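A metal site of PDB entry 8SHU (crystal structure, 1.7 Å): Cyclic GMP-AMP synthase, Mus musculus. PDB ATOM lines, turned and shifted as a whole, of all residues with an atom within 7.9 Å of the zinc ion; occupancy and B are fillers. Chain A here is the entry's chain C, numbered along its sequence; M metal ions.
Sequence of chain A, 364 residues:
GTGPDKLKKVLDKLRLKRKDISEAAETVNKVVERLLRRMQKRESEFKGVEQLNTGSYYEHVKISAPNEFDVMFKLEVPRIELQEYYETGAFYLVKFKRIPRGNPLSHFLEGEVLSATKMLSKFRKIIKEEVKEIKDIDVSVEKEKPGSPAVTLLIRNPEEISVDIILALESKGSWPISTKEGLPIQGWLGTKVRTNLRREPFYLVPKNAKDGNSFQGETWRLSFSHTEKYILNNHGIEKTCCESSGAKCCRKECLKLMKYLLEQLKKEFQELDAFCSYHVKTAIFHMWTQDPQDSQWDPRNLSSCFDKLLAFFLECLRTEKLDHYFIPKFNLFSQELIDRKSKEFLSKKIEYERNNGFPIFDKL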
ATOM      1  N   LEU A 232     -19.415  13.478  -2.649  1.00  0.00           N
ATOM      2  CA  LEU A 232     -19.511  14.323  -3.835  1.00  0.00           C
ATOM      3  C   LEU A 232     -20.896  14.237  -4.480  1.00  0.00           C
ATOM      4  O   LEU A 232     -21.367  15.214  -5.034  1.00  0.00           O
ATOM      5  CB  LEU A 232     -18.437  13.931  -4.846  1.00  0.00           C
ATOM      6  CG  LEU A 232     -17.145  14.753  -4.783  1.00  0.00           C
ATOM      7  CD1 LEU A 232     -17.371  16.127  -5.347  1.00  0.00           C
ATOM      8  CD2 LEU A 232     -16.597  14.863  -3.377  1.00  0.00           C
ATOM      9  N   ASN A 233     -21.467  13.035  -4.546  1.00  0.00           N
ATOM     10  CA  ASN A 233     -22.718  12.822  -5.254  1.00  0.00           C
ATOM     11  C   ASN A 233     -23.949  13.054  -4.354  1.00  0.00           C
ATOM     12  O   ASN A 233     -25.056  13.002  -4.862  1.00  0.00           O
ATOM     13  CB  ASN A 233     -22.715  11.456  -5.946  1.00  0.00           C
ATOM     14  CG  ASN A 233     -21.721  11.404  -7.098  1.00  0.00           C
ATOM     15  OD1 ASN A 233     -21.252  12.437  -7.584  1.00  0.00           O
ATOM     16  ND2 ASN A 233     -21.363  10.210  -7.545  1.00  0.00           N
ATOM     17  N   ASN A 234     -23.752  13.265  -3.053  1.00  0.00           N
ATOM     18  CA  ASN A 234     -24.781  13.512  -2.032  1.00  0.00           C
ATOM     19  C   ASN A 234     -24.344  14.627  -1.103  1.00  0.00           C
ATOM     20  O   ASN A 234     -24.141  14.431   0.102  1.00  0.00           O
ATOM     21  CB  ASN A 234     -25.045  12.253  -1.207  1.00  0.00           C
ATOM     22  CG  ASN A 234     -25.476  11.095  -2.063  1.00  0.00           C
ATOM     23  OD1 ASN A 234     -26.672  10.839  -2.176  1.00  0.00           O
ATOM     24  ND2 ASN A 234     -24.524  10.376  -2.653  1.00  0.00           N
ATOM     25  N   HIS A 235     -24.110  15.830  -1.651  1.00  0.00           N
ATOM     26  CA  HIS A 235     -23.293  16.824  -1.018  1.00  0.00           C
ATOM     27  C   HIS A 235     -24.100  17.950  -0.372  1.00  0.00           C
ATOM     28  O   HIS A 235     -23.521  18.878   0.154  1.00  0.00           O
ATOM     29  CB  HIS A 235     -22.323  17.422  -2.054  1.00  0.00           C
ATOM     30  CG  HIS A 235     -23.084  17.986  -3.205  1.00  0.00           C
ATOM     31  ND1 HIS A 235     -22.963  17.474  -4.469  1.00  0.00           N
ATOM     32  CD2 HIS A 235     -24.015  18.967  -3.253  1.00  0.00           C
ATOM     33  CE1 HIS A 235     -23.799  18.143  -5.280  1.00  0.00           C
ATOM     34  NE2 HIS A 235     -24.428  19.042  -4.563  1.00  0.00           N
ATOM     35  N   GLY A 236     -25.422  17.865  -0.426  1.00  0.00           N
ATOM     36  CA  GLY A 236     -26.251  18.962   0.101  1.00  0.00           C
ATOM     37  C   GLY A 236     -26.798  18.722   1.510  1.00  0.00           C
ATOM     38  O   GLY A 236     -26.898  17.581   1.958  1.00  0.00           O
ATOM     39  N   ILE A 237     -27.190  19.789   2.195  1.00  0.00           N
ATOM     40  CA  ILE A 237     -27.973  19.602   3.409  1.00  0.00           C
ATOM     41  C   ILE A 237     -29.385  19.132   3.007  1.00  0.00           C
ATOM     42  O   ILE A 237     -29.974  18.323   3.707  1.00  0.00           O
ATOM     43  CB  ILE A 237     -27.963  20.856   4.300  1.00  0.00           C
ATOM     44  CG1 ILE A 237     -28.591  20.576   5.665  1.00  0.00           C
ATOM     45  CG2 ILE A 237     -28.623  22.041   3.593  1.00  0.00           C
ATOM     46  CD1 ILE A 237     -28.104  21.563   6.696  1.00  0.00           C
ATOM     47  N   GLU A 238     -29.934  19.625   1.901  1.00  0.00           N
ATOM     48  CA  GLU A 238     -31.172  19.105   1.356  1.00  0.00           C
ATOM     49  C   GLU A 238     -30.879  17.900   0.466  1.00  0.00           C
ATOM     50  O   GLU A 238     -29.920  17.826  -0.304  1.00  0.00           O
ATOM     51  CB  GLU A 238     -31.930  20.147   0.538  1.00  0.00           C
ATOM     52  CG  GLU A 238     -32.309  21.365   1.352  1.00  0.00           C
ATOM     53  CD  GLU A 238     -33.382  22.230   0.711  1.00  0.00           C
ATOM     54  OE1 GLU A 238     -33.975  21.795  -0.301  1.00  0.00           O
ATOM     55  OE2 GLU A 238     -33.679  23.278   1.279  1.00  0.00           O
ATOM     56  N   THR A 240     -32.407  16.915  -2.007  1.00  0.00           N
ATOM     57  CA  THR A 240     -32.693  17.173  -3.397  1.00  0.00           C
ATOM     58  C   THR A 240     -31.679  18.122  -4.056  1.00  0.00           C
ATOM     59  O   THR A 240     -31.870  18.472  -5.196  1.00  0.00           O
ATOM     60  CB  THR A 240     -34.077  17.771  -3.544  1.00  0.00           C
ATOM     61  OG1 THR A 240     -34.186  18.959  -2.769  1.00  0.00           O
ATOM     62  CG2 THR A 240     -35.154  16.790  -3.126  1.00  0.00           C
ATOM     63  N   CYS A 241     -30.618  18.512  -3.341  1.00  0.00           N
ATOM     64  CA  CYS A 241     -29.592  19.375  -3.907  1.00  0.00           C
ATOM     65  C   CYS A 241     -29.072  18.763  -5.209  1.00  0.00           C
ATOM     66  O   CYS A 241     -28.632  17.598  -5.273  1.00  0.00           O
ATOM     67  CB  CYS A 241     -28.461  19.579  -2.893  1.00  0.00           C
ATOM     68  SG  CYS A 241     -27.325  20.911  -3.362  1.00  0.00           S
ATOM     69  N   CYS A 242     -29.114  19.592  -6.254  1.00  0.00           N
ATOM     70  CA  CYS A 242     -28.712  19.211  -7.607  1.00  0.00           C
ATOM     71  C   CYS A 242     -29.511  18.077  -8.242  1.00  0.00           C
ATOM     72  O   CYS A 242     -29.109  17.551  -9.274  1.00  0.00           O
ATOM     73  CB  CYS A 242     -27.200  18.908  -7.671  1.00  0.00           C
ATOM     74  SG  CYS A 242     -26.188  20.374  -7.319  1.00  0.00           S
ATOM     75  N   GLU A 243     -30.689  17.725  -7.724  1.00  0.00           N
ATOM     76  CA  GLU A 243     -31.550  16.763  -8.396  1.00  0.00           C
ATOM     77  C   GLU A 243     -32.569  17.492  -9.274  1.00  0.00           C
ATOM     78  O   GLU A 243     -32.755  18.689  -9.149  1.00  0.00           O
ATOM     79  CB  GLU A 243     -32.327  15.937  -7.367  1.00  0.00           C
ATOM     80  CG  GLU A 243     -31.469  14.973  -6.543  1.00  0.00           C
ATOM     81  CD  GLU A 243     -32.290  14.069  -5.613  1.00  0.00           C
ATOM     82  OE1 GLU A 243     -33.495  14.348  -5.537  1.00  0.00           O
ATOM     83  OE2 GLU A 243     -31.748  13.071  -5.093  1.00  0.00           O
ATOM     84  N   ALA A 247     -32.770  22.030  -6.259  1.00  0.00           N
ATOM     85  CA  ALA A 247     -32.096  23.266  -6.652  1.00  0.00           C
ATOM     86  C   ALA A 247     -30.621  22.954  -6.893  1.00  0.00           C
ATOM     87  O   ALA A 247     -30.025  22.302  -6.031  1.00  0.00           O
ATOM     88  CB  ALA A 247     -32.196  24.248  -5.514  1.00  0.00           C
ATOM     89  N   LYS A 248     -30.059  23.509  -7.968  1.00  0.00           N
ATOM     90  CA  LYS A 248     -28.627  23.435  -8.233  1.00  0.00           C
ATOM     91  C   LYS A 248     -27.866  24.211  -7.151  1.00  0.00           C
ATOM     92  O   LYS A 248     -28.324  25.288  -6.740  1.00  0.00           O
ATOM     93  CB  LYS A 248     -28.295  23.990  -9.621  1.00  0.00           C
ATOM     94  CG  LYS A 248     -28.365  22.973 -10.741  1.00  0.00           C
ATOM     95  CD  LYS A 248     -27.214  21.979 -10.704  1.00  0.00           C
ATOM     96  CE  LYS A 248     -25.879  22.591 -11.093  1.00  0.00           C
ATOM     97  NZ  LYS A 248     -24.715  22.004 -10.375  1.00  0.00           N
ATOM     98  N   CYS A 249     -26.676  23.692  -6.772  1.00  0.00           N
ATOM     99  CA  CYS A 249     -25.684  24.469  -6.065  1.00  0.00           C
ATOM    100  C   CYS A 249     -24.410  24.576  -6.916  1.00  0.00           C
ATOM    101  O   CYS A 249     -24.341  23.986  -7.980  1.00  0.00           O
ATOM    102  CB  CYS A 249     -25.376  23.876  -4.695  1.00  0.00           C
ATOM    103  SG  CYS A 249     -24.367  22.375  -4.785  1.00  0.00           S
ATOM    104  N   CYS A 250     -23.389  25.289  -6.397  1.00  0.00           N
ATOM    105  CA  CYS A 250     -22.146  25.463  -7.123  1.00  0.00           C
ATOM    106  C   CYS A 250     -20.981  24.771  -6.391  1.00  0.00           C
ATOM    107  O   CYS A 250     -19.811  25.033  -6.661  1.00  0.00           O
ATOM    108  CB  CYS A 250     -21.817  26.931  -7.373  1.00  0.00           C
ATOM    109  SG  CYS A 250     -21.417  27.857  -5.887  1.00  0.00           S
ATOM    110  N   ARG A 251     -21.263  23.766  -5.568  1.00  0.00           N
ATOM    111  CA  ARG A 251     -20.210  23.065  -4.819  1.00  0.00           C
ATOM    112  C   ARG A 251     -19.231  22.364  -5.758  1.00  0.00           C
ATOM    113  O   ARG A 251     -17.999  22.544  -5.602  1.00  0.00           O
ATOM    114  CB  ARG A 251     -20.818  22.058  -3.832  1.00  0.00           C
ATOM    115  CG  ARG A 251     -21.416  22.685  -2.589  1.00  0.00           C
ATOM    116  CD  ARG A 251     -21.839  21.582  -1.620  1.00  0.00           C
ATOM    117  NE  ARG A 251     -22.451  22.125  -0.421  1.00  0.00           N
ATOM    118  CZ  ARG A 251     -23.780  22.171  -0.265  1.00  0.00           C
ATOM    119  NH1 ARG A 251     -24.577  22.015  -1.320  1.00  0.00           N
ATOM    120  NH2 ARG A 251     -24.257  22.396   0.939  1.00  0.00           N
ATOM    121  N   LYS A 252     -19.738  21.542  -6.681  1.00  0.00           N
ATOM    122  CA  LYS A 252     -18.829  20.798  -7.541  1.00  0.00           C
ATOM    123  C   LYS A 252     -18.131  21.724  -8.525  1.00  0.00           C
ATOM    124  O   LYS A 252     -16.994  21.458  -8.938  1.00  0.00           O
ATOM    125  CB  LYS A 252     -19.555  19.668  -8.276  1.00  0.00           C
ATOM    126  CG  LYS A 252     -20.174  18.591  -7.378  1.00  0.00           C
ATOM    127  CD  LYS A 252     -20.860  17.409  -8.103  1.00  0.00           C
ATOM    128  CE  LYS A 252     -20.108  16.101  -8.048  1.00  0.00           C
ATOM    129  NZ  LYS A 252     -20.958  14.952  -8.496  1.00  0.00           N
ATOM    130  N   GLU A 253     -18.823  22.771  -8.964  1.00  0.00           N
ATOM    131  CA  GLU A 253     -18.245  23.745  -9.876  1.00  0.00           C
ATOM    132  C   GLU A 253     -17.014  24.392  -9.248  1.00  0.00           C
ATOM    133  O   GLU A 253     -15.966  24.553  -9.917  1.00  0.00           O
ATOM    134  CB  GLU A 253     -19.323  24.741 -10.298  1.00  0.00           C
ATOM    135  CG  GLU A 253     -20.342  24.103 -11.189  1.00  0.00           C
ATOM    136  CD  GLU A 253     -21.427  23.289 -10.499  1.00  0.00           C
ATOM    137  OE1 GLU A 253     -21.458  23.226  -9.260  1.00  0.00           O
ATOM    138  OE2 GLU A 253     -22.215  22.694 -11.259  1.00  0.00           O
ATOM    139  N   ASP A 294     -26.944  24.819   1.777  1.00  0.00           N
ATOM    140  CA  ASP A 294     -27.028  24.844   0.335  1.00  0.00           C
ATOM    141  C   ASP A 294     -27.136  26.295  -0.145  1.00  0.00           C
ATOM    142  O   ASP A 294     -26.633  26.606  -1.214  1.00  0.00           O
ATOM    143  CB  ASP A 294     -28.176  24.029  -0.253  1.00  0.00           C
ATOM    144  CG  ASP A 294     -28.102  22.546   0.102  1.00  0.00           C
ATOM    145  OD1 ASP A 294     -26.987  22.091   0.474  1.00  0.00           O
ATOM    146  OD2 ASP A 294     -29.153  21.854  -0.047  1.00  0.00           O
ATOM    147  N   TRP A 297     -24.098  28.046  -1.170  1.00  0.00           N
ATOM    148  CA  TRP A 297     -23.524  27.610  -2.422  1.00  0.00           C
ATOM    149  C   TRP A 297     -24.507  27.764  -3.570  1.00  0.00           C
ATOM    150  O   TRP A 297     -24.514  26.982  -4.539  1.00  0.00           O
ATOM    151  CB  TRP A 297     -23.040  26.145  -2.291  1.00  0.00           C
ATOM    152  CG  TRP A 297     -21.995  26.013  -1.228  1.00  0.00           C
ATOM    153  CD1 TRP A 297     -22.217  25.832   0.090  1.00  0.00           C
ATOM    154  CD2 TRP A 297     -20.569  26.086  -1.390  1.00  0.00           C
ATOM    155  NE1 TRP A 297     -21.044  25.808   0.789  1.00  0.00           N
ATOM    156  CE2 TRP A 297     -20.012  25.988  -0.097  1.00  0.00           C
ATOM    157  CE3 TRP A 297     -19.711  26.275  -2.481  1.00  0.00           C
ATOM    158  CZ2 TRP A 297     -18.632  26.015   0.139  1.00  0.00           C
ATOM    159  CZ3 TRP A 297     -18.362  26.335  -2.246  1.00  0.00           C
ATOM    160  CH2 TRP A 297     -17.821  26.160  -0.967  1.00  0.00           C
HETATM  161 ZN    ZN M   1     -25.795  20.538  -5.090  1.00  0.00          ZN
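SG of Cys 249 lies close to NH1 of Arg 251 (3.5 Å). SG of Cys 241 sits close to NH1 of Arg 251. The side-chain sulfur of Cys 242 sits close to the side-chain amino group of Lys 248 (3.8 Å). A ring nitrogen (ND1) of His 235 lies within hydrogen-bond range of the backbone carbonyl oxygen (O) of Leu 232, 2.8 Å away. O of His 235 sits close to NE of Arg 251. N of Cys 242 sits at hydrogen-bond distance from O of Ala 247, at 2.9 Å.
Of the 20 residues printed, 4 come within 4 Å of the zinc ion. The nearest printed residue that does not touch the zinc ion is Arg 251 (4.2 Å).
A ring nitrogen (NE2) of His 235 binds the zinc ion (2.1 Å). The zinc ion is bound by SG of Cys 242 (2.3 Å). SG of Cys 241 binds the zinc ion (2.3 Å). The zinc ion is bound by SG of Cys 249, at 2.3 Å.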
